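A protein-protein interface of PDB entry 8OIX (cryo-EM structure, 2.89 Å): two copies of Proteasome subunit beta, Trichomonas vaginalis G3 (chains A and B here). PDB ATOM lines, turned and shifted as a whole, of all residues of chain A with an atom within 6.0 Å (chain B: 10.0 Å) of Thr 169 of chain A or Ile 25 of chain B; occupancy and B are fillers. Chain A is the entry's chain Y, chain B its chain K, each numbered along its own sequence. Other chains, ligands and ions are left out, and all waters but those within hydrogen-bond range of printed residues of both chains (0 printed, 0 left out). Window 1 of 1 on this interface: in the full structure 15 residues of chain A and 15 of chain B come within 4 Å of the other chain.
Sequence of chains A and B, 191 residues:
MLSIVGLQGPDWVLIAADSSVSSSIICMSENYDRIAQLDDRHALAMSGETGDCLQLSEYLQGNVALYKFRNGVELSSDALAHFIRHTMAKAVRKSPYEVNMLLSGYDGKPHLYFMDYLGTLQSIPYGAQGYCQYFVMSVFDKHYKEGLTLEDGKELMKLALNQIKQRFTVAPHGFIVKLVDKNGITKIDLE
The backbone carbonyl oxygen (O) of Ile 25 of chain B sits at hydrogen-bond distance from the backbone NH (N) of Thr 169 of chain A (2.8 Å).
N of Cys 27 of chain B lies within hydrogen-bond range of O of Arg 167 of chain A, 2.5 Å away.
The guanidinium group of Arg 167 of chain A is in hydrogen-bond range of the backbone carbonyl oxygen of Met 28 of chain B.
The backbone carbonyl oxygen of Arg 167 of chain A lies close to the backbone carbonyl oxygen of Ile 25 of chain B, 3.4 Å away.
The backbone carbonyl oxygen (O) of Val 21 of chain B sits at hydrogen-bond distance from the backbone NH (N) of Met 28 of chain B (3.0 Å).
O of Ser 24 of chain B lies within hydrogen-bond range of OG of Ser 22 of chain B (3.3 Å).
The side-chain sulfur (SG) of Cys 27 of chain B lies within hydrogen-bond range of the backbone carbonyl oxygen (O) of Ser 29 of chain B (3.3 Å).
Ile 25 of chain B touches Tyr 131 of chain A.
Phe 135 of chain A touches Ile 25 of chain B.
Ile 26 of chain B touches Arg 167 of chain A.
Phe 168 of chain A touches Ile 25 of chain B.
Thr 169 of chain A touches Ser 22 of chain B (CG2 to OG, 3.2 Å).
Thr 169 of chain A touches Ser 24 of chain B (CG2 to O, 3.4 Å).
CG2 of Thr 169 of chain A touches O of Ile 26 of chain B, at 3.4 Å.
Cys 27 of chain B touches Thr 169 of chain A (N to CG2, 3.8 Å).
Thr 169 of chain A touches just these residues of chain B: Ser 22, Ser 24, Ile 25, Ile 26 and Cys 27.
Of chain A, only Tyr 131, Phe 135, Arg 167, Phe 168 and Thr 169 come within 4 Å of Ile 25 of chain B.
Of chain B, only Ile 25 (3.3 Å) comes within 4 Å of Phe 168 of chain A.
No residue of chain B comes within 4 Å of Val 170 of chain A.
Of the printed residues of chain B, Phe 135 of chain A touches Ile 25.
Of the printed residues of chain B, Arg 167 of chain A touches Ile 25, Ile 26, Cys 27 and Met 28.
Printed residues of chain A within 4 Å of Ser 22 of chain B: Thr 169 (3.2 Å).
Tyr 134 of chain A touches none of the printed residues of chain B.
The nearest residue of chain B that does not touch Thr 169 of chain A is Val 170 of chain B (4.1 Å).
Of the 23 printed residues of chain B, 6 touch a printed residue of chain A.
Printed residues of chain A that touch a printed residue of chain B: Tyr 131, Phe 135, Arg 167, Phe 168 and Thr 169.
Hydrophobic or aromatic side chains of chain A within 4 Å of the printed part of chain B: Tyr 131, Phe 135 and Phe 168.
Among the printed residues, 12 pairs touch across the chains.
4 positions are printed for both chains.
Of the 12 pairs that touch across the chains among the printed residues, none has its exchanged pair printed and touching as well.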
ATOM      1  N   TYR A 131      13.516  -4.169 -25.006  1.00  0.00           N
ATOM      2  CA  TYR A 131      13.207  -2.894 -24.370  1.00  0.00           C
ATOM      3  C   TYR A 131      14.456  -2.161 -23.902  1.00  0.00           C
ATOM      4  O   TYR A 131      14.376  -0.972 -23.567  1.00  0.00           O
ATOM      5  CB  TYR A 131      12.258  -3.105 -23.190  1.00  0.00           C
ATOM      6  CG  TYR A 131      10.862  -3.513 -23.598  1.00  0.00           C
ATOM      7  CD1 TYR A 131       9.987  -2.593 -24.157  1.00  0.00           C
ATOM      8  CD2 TYR A 131      10.420  -4.816 -23.424  1.00  0.00           C
ATOM      9  CE1 TYR A 131       8.710  -2.959 -24.533  1.00  0.00           C
ATOM     10  CE2 TYR A 131       9.145  -5.191 -23.797  1.00  0.00           C
ATOM     11  CZ  TYR A 131       8.295  -4.259 -24.352  1.00  0.00           C
ATOM     12  OH  TYR A 131       7.024  -4.628 -24.725  1.00  0.00           O
ATOM     13  N   TYR A 134      15.348   1.406 -25.084  1.00  0.00           N
ATOM     14  CA  TYR A 134      14.734   2.546 -24.415  1.00  0.00           C
ATOM     15  C   TYR A 134      15.594   3.044 -23.269  1.00  0.00           C
ATOM     16  O   TYR A 134      15.493   4.213 -22.888  1.00  0.00           O
ATOM     17  CB  TYR A 134      13.340   2.173 -23.907  1.00  0.00           C
ATOM     18  CG  TYR A 134      12.354   1.878 -25.013  1.00  0.00           C
ATOM     19  CD1 TYR A 134      11.726   2.907 -25.697  1.00  0.00           C
ATOM     20  CD2 TYR A 134      12.056   0.573 -25.373  1.00  0.00           C
ATOM     21  CE1 TYR A 134      10.827   2.645 -26.708  1.00  0.00           C
ATOM     22  CE2 TYR A 134      11.157   0.302 -26.383  1.00  0.00           C
ATOM     23  CZ  TYR A 134      10.546   1.342 -27.048  1.00  0.00           C
ATOM     24  OH  TYR A 134       9.648   1.079 -28.057  1.00  0.00           O
ATOM     25  N   PHE A 135      16.476   2.195 -22.755  1.00  0.00           N
ATOM     26  CA  PHE A 135      17.339   2.531 -21.640  1.00  0.00           C
ATOM     27  C   PHE A 135      18.770   2.818 -22.052  1.00  0.00           C
ATOM     28  O   PHE A 135      19.472   3.518 -21.322  1.00  0.00           O
ATOM     29  CB  PHE A 135      17.344   1.392 -20.614  1.00  0.00           C
ATOM     30  CG  PHE A 135      15.989   1.069 -20.062  1.00  0.00           C
ATOM     31  CD1 PHE A 135      15.498   1.744 -18.960  1.00  0.00           C
ATOM     32  CD2 PHE A 135      15.207   0.088 -20.643  1.00  0.00           C
ATOM     33  CE1 PHE A 135      14.253   1.447 -18.449  1.00  0.00           C
ATOM     34  CE2 PHE A 135      13.960  -0.211 -20.138  1.00  0.00           C
ATOM     35  CZ  PHE A 135      13.483   0.470 -19.039  1.00  0.00           C
ATOM     36  N   ILE A 164      20.412  -1.120 -18.085  1.00  0.00           N
ATOM     37  CA  ILE A 164      19.430  -2.188 -18.264  1.00  0.00           C
ATOM     38  C   ILE A 164      19.149  -2.870 -16.933  1.00  0.00           C
ATOM     39  O   ILE A 164      17.994  -3.108 -16.564  1.00  0.00           O
ATOM     40  CB  ILE A 164      19.919  -3.209 -19.305  1.00  0.00           C
ATOM     41  CG1 ILE A 164      20.203  -2.533 -20.634  1.00  0.00           C
ATOM     42  CG2 ILE A 164      18.877  -4.290 -19.506  1.00  0.00           C
ATOM     43  CD1 ILE A 164      20.925  -3.426 -21.594  1.00  0.00           C
ATOM     44  N   ARG A 167      17.304  -0.001 -14.377  1.00  0.00           N
ATOM     45  CA  ARG A 167      16.030   0.633 -14.686  1.00  0.00           C
ATOM     46  C   ARG A 167      15.027  -0.275 -15.382  1.00  0.00           C
ATOM     47  O   ARG A 167      13.822  -0.030 -15.269  1.00  0.00           O
ATOM     48  CB  ARG A 167      16.255   1.874 -15.555  1.00  0.00           C
ATOM     49  CG  ARG A 167      16.896   3.023 -14.814  1.00  0.00           C
ATOM     50  CD  ARG A 167      16.037   3.470 -13.646  1.00  0.00           C
ATOM     51  NE  ARG A 167      16.703   4.492 -12.849  1.00  0.00           N
ATOM     52  CZ  ARG A 167      16.281   4.911 -11.665  1.00  0.00           C
ATOM     53  NH1 ARG A 167      15.199   4.402 -11.098  1.00  0.00           N
ATOM     54  NH2 ARG A 167      16.963   5.859 -11.030  1.00  0.00           N
ATOM     55  N   PHE A 168      15.474  -1.307 -16.090  1.00  0.00           N
ATOM     56  CA  PHE A 168      14.550  -2.215 -16.758  1.00  0.00           C
ATOM     57  C   PHE A 168      13.928  -3.140 -15.719  1.00  0.00           C
ATOM     58  O   PHE A 168      14.646  -3.790 -14.951  1.00  0.00           O
ATOM     59  CB  PHE A 168      15.272  -3.010 -17.844  1.00  0.00           C
ATOM     60  CG  PHE A 168      14.357  -3.776 -18.759  1.00  0.00           C
ATOM     61  CD1 PHE A 168      12.995  -3.528 -18.780  1.00  0.00           C
ATOM     62  CD2 PHE A 168      14.866  -4.752 -19.597  1.00  0.00           C
ATOM     63  CE1 PHE A 168      12.161  -4.236 -19.619  1.00  0.00           C
ATOM     64  CE2 PHE A 168      14.037  -5.464 -20.438  1.00  0.00           C
ATOM     65  CZ  PHE A 168      12.682  -5.205 -20.448  1.00  0.00           C
ATOM     66  N   THR A 169      12.593  -3.176 -15.681  1.00  0.00           N
ATOM     67  CA  THR A 169      11.886  -4.001 -14.703  1.00  0.00           C
ATOM     68  C   THR A 169      12.328  -5.454 -14.787  1.00  0.00           C
ATOM     69  O   THR A 169      12.697  -6.065 -13.777  1.00  0.00           O
ATOM     70  CB  THR A 169      10.380  -3.896 -14.922  1.00  0.00           C
ATOM     71  OG1 THR A 169      10.097  -3.971 -16.324  1.00  0.00           O
ATOM     72  CG2 THR A 169       9.875  -2.584 -14.394  1.00  0.00           C
ATOM     73  N   VAL A 170      12.300  -6.025 -15.988  1.00  0.00           N
ATOM     74  CA  VAL A 170      12.811  -7.372 -16.187  1.00  0.00           C
ATOM     75  C   VAL A 170      14.306  -7.240 -16.418  1.00  0.00           C
ATOM     76  O   VAL A 170      14.776  -7.225 -17.561  1.00  0.00           O
ATOM     77  CB  VAL A 170      12.112  -8.081 -17.361  1.00  0.00           C
ATOM     78  CG1 VAL A 170      12.531  -9.542 -17.425  1.00  0.00           C
ATOM     79  CG2 VAL A 170      10.602  -7.959 -17.229  1.00  0.00           C
ATOM     80  N   ALA A 171      15.058  -7.131 -15.332  1.00  0.00           N
ATOM     81  CA  ALA A 171      16.494  -6.933 -15.426  1.00  0.00           C
ATOM     82  C   ALA A 171      17.175  -8.256 -15.742  1.00  0.00           C
ATOM     83  O   ALA A 171      17.020  -9.217 -14.978  1.00  0.00           O
ATOM     84  CB  ALA A 171      17.041  -6.359 -14.127  1.00  0.00           C
ATOM     85  N   MET B   1       2.333  -9.040  -9.574  1.00  0.00           N
ATOM     86  CA  MET B   1       3.156 -10.242  -9.493  1.00  0.00           C
ATOM     87  C   MET B   1       4.443  -9.968  -8.724  1.00  0.00           C
ATOM     88  O   MET B   1       5.522 -10.403  -9.125  1.00  0.00           O
ATOM     89  CB  MET B   1       3.479 -10.767 -10.892  1.00  0.00           C
ATOM     90  N   LEU B   2       4.318  -9.242  -7.619  1.00  0.00           N
ATOM     91  CA  LEU B   2       5.463  -8.862  -6.806  1.00  0.00           C
ATOM     92  C   LEU B   2       5.745  -9.921  -5.749  1.00  0.00           C
ATOM     93  O   LEU B   2       4.837 -10.585  -5.245  1.00  0.00           O
ATOM     94  CB  LEU B   2       5.226  -7.504  -6.152  1.00  0.00           C
ATOM     95  CG  LEU B   2       4.817  -6.444  -7.172  1.00  0.00           C
ATOM     96  CD1 LEU B   2       4.507  -5.131  -6.493  1.00  0.00           C
ATOM     97  CD2 LEU B   2       5.924  -6.266  -8.201  1.00  0.00           C
ATOM     98  N   ASP B  18       9.486  -7.480  -2.240  1.00  0.00           N
ATOM     99  CA  ASP B  18      10.188  -6.865  -3.356  1.00  0.00           C
ATOM    100  C   ASP B  18      10.307  -5.366  -3.119  1.00  0.00           C
ATOM    101  O   ASP B  18       9.299  -4.669  -2.968  1.00  0.00           O
ATOM    102  CB  ASP B  18       9.441  -7.151  -4.659  1.00  0.00           C
ATOM    103  CG  ASP B  18      10.139  -6.581  -5.881  1.00  0.00           C
ATOM    104  OD1 ASP B  18      11.255  -6.039  -5.747  1.00  0.00           O
ATOM    105  OD2 ASP B  18       9.565  -6.678  -6.986  1.00  0.00           O
ATOM    106  N   SER B  20      11.627  -3.224  -5.254  1.00  0.00           N
ATOM    107  CA  SER B  20      11.694  -2.524  -6.529  1.00  0.00           C
ATOM    108  C   SER B  20      10.284  -2.126  -6.944  1.00  0.00           C
ATOM    109  O   SER B  20       9.464  -2.987  -7.277  1.00  0.00           O
ATOM    110  CB  SER B  20      12.348  -3.402  -7.593  1.00  0.00           C
ATOM    111  OG  SER B  20      13.629  -3.837  -7.175  1.00  0.00           O
ATOM    112  N   VAL B  21      10.000  -0.829  -6.921  1.00  0.00           N
ATOM    113  CA  VAL B  21       8.740  -0.317  -7.448  1.00  0.00           C
ATOM    114  C   VAL B  21       8.930  -0.074  -8.936  1.00  0.00           C
ATOM    115  O   VAL B  21      10.048   0.152  -9.412  1.00  0.00           O
ATOM    116  CB  VAL B  21       8.278   0.958  -6.713  1.00  0.00           C
ATOM    117  CG1 VAL B  21       8.915   2.194  -7.319  1.00  0.00           C
ATOM    118  CG2 VAL B  21       6.767   1.061  -6.743  1.00  0.00           C
ATOM    119  N   SER B  22       7.838  -0.139  -9.690  1.00  0.00           N
ATOM    120  CA  SER B  22       7.960  -0.106 -11.136  1.00  0.00           C
ATOM    121  C   SER B  22       6.802   0.647 -11.768  1.00  0.00           C
ATOM    122  O   SER B  22       5.683   0.657 -11.247  1.00  0.00           O
ATOM    123  CB  SER B  22       8.016  -1.526 -11.699  1.00  0.00           C
ATOM    124  OG  SER B  22       7.245  -1.631 -12.882  1.00  0.00           O
ATOM    125  N   SER B  23       7.095   1.284 -12.900  1.00  0.00           N
ATOM    126  CA  SER B  23       6.092   1.867 -13.784  1.00  0.00           C
ATOM    127  C   SER B  23       6.351   1.316 -15.179  1.00  0.00           C
ATOM    128  O   SER B  23       7.332   1.699 -15.825  1.00  0.00           O
ATOM    129  CB  SER B  23       6.156   3.393 -13.770  1.00  0.00           C
ATOM    130  OG  SER B  23       5.248   3.952 -14.702  1.00  0.00           O
ATOM    131  N   SER B  24       5.479   0.418 -15.639  1.00  0.00           N
ATOM    132  CA  SER B  24       5.588  -0.216 -16.957  1.00  0.00           C
ATOM    133  C   SER B  24       6.903  -0.985 -16.994  1.00  0.00           C
ATOM    134  O   SER B  24       7.097  -1.879 -16.152  1.00  0.00           O
ATOM    135  CB  SER B  24       5.404   0.844 -18.046  1.00  0.00           C
ATOM    136  OG  SER B  24       5.445   0.261 -19.337  1.00  0.00           O
ATOM    137  N   ILE B  25       7.819  -0.695 -17.925  1.00  0.00           N
ATOM    138  CA  ILE B  25       9.089  -1.407 -18.010  1.00  0.00           C
ATOM    139  C   ILE B  25      10.185  -0.742 -17.192  1.00  0.00           C
ATOM    140  O   ILE B  25      11.343  -1.175 -17.258  1.00  0.00           O
ATOM    141  CB  ILE B  25       9.567  -1.532 -19.472  1.00  0.00           C
ATOM    142  CG1 ILE B  25       9.883  -0.151 -20.048  1.00  0.00           C
ATOM    143  CG2 ILE B  25       8.520  -2.239 -20.314  1.00  0.00           C
ATOM    144  CD1 ILE B  25      10.520  -0.189 -21.418  1.00  0.00           C
ATOM    145  N   ILE B  26       9.862   0.295 -16.426  1.00  0.00           N
ATOM    146  CA  ILE B  26      10.849   1.106 -15.726  1.00  0.00           C
ATOM    147  C   ILE B  26      10.819   0.769 -14.243  1.00  0.00           C
ATOM    148  O   ILE B  26       9.752   0.773 -13.621  1.00  0.00           O
ATOM    149  CB  ILE B  26      10.580   2.603 -15.932  1.00  0.00           C
ATOM    150  CG1 ILE B  26      10.076   2.856 -17.348  1.00  0.00           C
ATOM    151  CG2 ILE B  26      11.842   3.387 -15.683  1.00  0.00           C
ATOM    152  CD1 ILE B  26       9.831   4.302 -17.637  1.00  0.00           C
ATOM    153  N   CYS B  27      11.992   0.482 -13.679  1.00  0.00           N
ATOM    154  CA  CYS B  27      12.144   0.301 -12.236  1.00  0.00           C
ATOM    155  C   CYS B  27      12.331   1.681 -11.618  1.00  0.00           C
ATOM    156  O   CYS B  27      13.442   2.209 -11.542  1.00  0.00           O
ATOM    157  CB  CYS B  27      13.316  -0.620 -11.924  1.00  0.00           C
ATOM    158  SG  CYS B  27      13.658  -0.830 -10.162  1.00  0.00           S
ATOM    159  N   MET B  28      11.220   2.279 -11.178  1.00  0.00           N
ATOM    160  CA  MET B  28      11.258   3.653 -10.682  1.00  0.00           C
ATOM    161  C   MET B  28      12.134   3.783  -9.444  1.00  0.00           C
ATOM    162  O   MET B  28      12.904   4.742  -9.317  1.00  0.00           O
ATOM    163  CB  MET B  28       9.841   4.143 -10.385  1.00  0.00           C
ATOM    164  CG  MET B  28       8.911   4.090 -11.579  1.00  0.00           C
ATOM    165  SD  MET B  28       9.399   5.212 -12.901  1.00  0.00           S
ATOM    166  CE  MET B  28       8.718   6.752 -12.300  1.00  0.00           C
ATOM    167  N   SER B  29      12.030   2.835  -8.517  1.00  0.00           N
ATOM    168  CA  SER B  29      12.800   2.875  -7.285  1.00  0.00           C
ATOM    169  C   SER B  29      13.278   1.475  -6.940  1.00  0.00           C
ATOM    170  O   SER B  29      12.639   0.480  -7.288  1.00  0.00           O
ATOM    171  CB  SER B  29      11.987   3.454  -6.120  1.00  0.00           C
ATOM    172  OG  SER B  29      12.757   3.497  -4.932  1.00  0.00           O
ATOM    173  N   GLU B  30      14.413   1.412  -6.249  1.00  0.00           N
ATOM    174  CA  GLU B  30      15.045   0.154  -5.878  1.00  0.00           C
ATOM    175  C   GLU B  30      14.989  -0.094  -4.376  1.00  0.00           C
ATOM    176  O   GLU B  30      15.555  -1.081  -3.895  1.00  0.00           O
ATOM    177  CB  GLU B  30      16.494   0.143  -6.371  1.00  0.00           C
ATOM    178  CG  GLU B  30      17.119  -1.231  -6.525  1.00  0.00           C
ATOM    179  CD  GLU B  30      18.470  -1.171  -7.208  1.00  0.00           C
ATOM    180  OE1 GLU B  30      18.669  -0.273  -8.053  1.00  0.00           O
ATOM    181  OE2 GLU B  30      19.334  -2.016  -6.896  1.00  0.00           O
ATOM    182  N   ARG B  34       7.602  -2.073   0.413  1.00  0.00           N
ATOM    183  CA  ARG B  34       6.292  -2.653   0.156  1.00  0.00           C
ATOM    184  C   ARG B  34       5.643  -3.227   1.407  1.00  0.00           C
ATOM    185  O   ARG B  34       4.437  -3.492   1.399  1.00  0.00           O
ATOM    186  CB  ARG B  34       6.408  -3.735  -0.915  1.00  0.00           C
ATOM    187  CG  ARG B  34       5.289  -3.713  -1.925  1.00  0.00           C
ATOM    188  CD  ARG B  34       5.600  -4.619  -3.096  1.00  0.00           C
ATOM    189  NE  ARG B  34       6.781  -4.172  -3.821  1.00  0.00           N
ATOM    190  CZ  ARG B  34       6.789  -3.166  -4.681  1.00  0.00           C
ATOM    191  NH1 ARG B  34       5.690  -2.489  -4.967  1.00  0.00           N
ATOM    192  NH2 ARG B  34       7.929  -2.833  -5.277  1.00  0.00           N
ATOM    193  N   THR B  50       1.101  -0.887  -7.100  1.00  0.00           N
ATOM    194  CA  THR B  50       1.599  -0.023  -6.034  1.00  0.00           C
ATOM    195  C   THR B  50       0.490   0.843  -5.454  1.00  0.00           C
ATOM    196  O   THR B  50       0.430   1.060  -4.239  1.00  0.00           O
ATOM    197  CB  THR B  50       2.740   0.850  -6.556  1.00  0.00           C
ATOM    198  OG1 THR B  50       3.744   0.018  -7.148  1.00  0.00           O
ATOM    199  CG2 THR B  50       3.360   1.647  -5.421  1.00  0.00           C
ATOM    200  N   PHE B 168      13.580 -16.818 -10.725  1.00  0.00           N
ATOM    201  CA  PHE B 168      12.436 -16.054 -11.206  1.00  0.00           C
ATOM    202  C   PHE B 168      12.891 -15.141 -12.339  1.00  0.00           C
ATOM    203  O   PHE B 168      13.847 -14.375 -12.177  1.00  0.00           O
ATOM    204  CB  PHE B 168      11.810 -15.253 -10.066  1.00  0.00           C
ATOM    205  CG  PHE B 168      10.477 -14.644 -10.400  1.00  0.00           C
ATOM    206  CD1 PHE B 168       9.773 -15.037 -11.526  1.00  0.00           C
ATOM    207  CD2 PHE B 168       9.930 -13.672  -9.583  1.00  0.00           C
ATOM    208  CE1 PHE B 168       8.552 -14.473 -11.830  1.00  0.00           C
ATOM    209  CE2 PHE B 168       8.710 -13.103  -9.880  1.00  0.00           C
ATOM    210  CZ  PHE B 168       8.020 -13.504 -11.006  1.00  0.00           C
ATOM    211  N   THR B 169      12.221 -15.246 -13.491  1.00  0.00           N
ATOM    212  CA  THR B 169      12.590 -14.445 -14.655  1.00  0.00           C
ATOM    213  C   THR B 169      12.595 -12.960 -14.322  1.00  0.00           C
ATOM    214  O   THR B 169      13.577 -12.255 -14.582  1.00  0.00           O
ATOM    215  CB  THR B 169      11.628 -14.721 -15.806  1.00  0.00           C
ATOM    216  OG1 THR B 169      10.287 -14.761 -15.307  1.00  0.00           O
ATOM    217  CG2 THR B 169      11.951 -16.047 -16.436  1.00  0.00           C
ATOM    218  N   VAL B 170      11.505 -12.468 -13.743  1.00  0.00           N
ATOM    219  CA  VAL B 170      11.460 -11.087 -13.286  1.00  0.00           C
ATOM    220  C   VAL B 170      12.060 -11.072 -11.890  1.00  0.00           C
ATOM    221  O   VAL B 170      11.341 -11.105 -10.886  1.00  0.00           O
ATOM    222  CB  VAL B 170      10.026 -10.528 -13.296  1.00  0.00           C
ATOM    223  CG1 VAL B 170      10.034  -9.037 -12.993  1.00  0.00           C
ATOM    224  CG2 VAL B 170       9.361 -10.803 -14.635  1.00  0.00           C
ATOM    225  N   ALA B 171      13.384 -11.037 -11.824  1.00  0.00           N
ATOM    226  CA  ALA B 171      14.077 -11.086 -10.548  1.00  0.00           C
ATOM    227  C   ALA B 171      14.024  -9.718  -9.883  1.00  0.00           C
ATOM    228  O   ALA B 171      14.487  -8.736 -10.476  1.00  0.00           O
ATOM    229  CB  ALA B 171      15.522 -11.521 -10.742  1.00  0.00           C
ATOM    230  N   PRO B 172      13.454  -9.602  -8.686  1.00  0.00           N
ATOM    231  CA  PRO B 172      13.483  -8.319  -7.979  1.00  0.00           C
ATOM    232  C   PRO B 172      14.912  -7.836  -7.790  1.00  0.00           C
ATOM    233  O   PRO B 172      15.805  -8.607  -7.430  1.00  0.00           O
ATOM    234  CB  PRO B 172      12.816  -8.643  -6.639  1.00  0.00           C
ATOM    235  CG  PRO B 172      11.919  -9.792  -6.953  1.00  0.00           C
ATOM    236  CD  PRO B 172      12.684 -10.616  -7.949  1.00  0.00           C
ATOM    237  N   HIS B 173      15.127  -6.545  -8.046  1.00  0.00           N
ATOM    238  CA  HIS B 173      16.464  -5.984  -7.905  1.00  0.00           C
ATOM    239  C   HIS B 173      16.938  -5.999  -6.461  1.00  0.00           C
ATOM    240  O   HIS B 173      18.136  -5.831  -6.211  1.00  0.00           O
ATOM    241  CB  HIS B 173      16.503  -4.559  -8.449  1.00  0.00           C
ATOM    242  CG  HIS B 173      17.785  -4.219  -9.141  1.00  0.00           C
ATOM    243  ND1 HIS B 173      18.950  -3.938  -8.460  1.00  0.00           N
ATOM    244  CD2 HIS B 173      18.086  -4.121 -10.455  1.00  0.00           C
ATOM    245  CE1 HIS B 173      19.913  -3.680  -9.326  1.00  0.00           C
ATOM    246  NE2 HIS B 173      19.414  -3.783 -10.545  1.00  0.00           N
ATOM    247  N   GLY B 174      16.030  -6.196  -5.516  1.00  0.00           N
ATOM    248  CA  GLY B 174      16.396  -6.308  -4.119  1.00  0.00           C
ATOM    249  C   GLY B 174      15.153  -6.563  -3.300  1.00  0.00           C
ATOM    250  O   GLY B 174      14.023  -6.451  -3.788  1.00  0.00           O
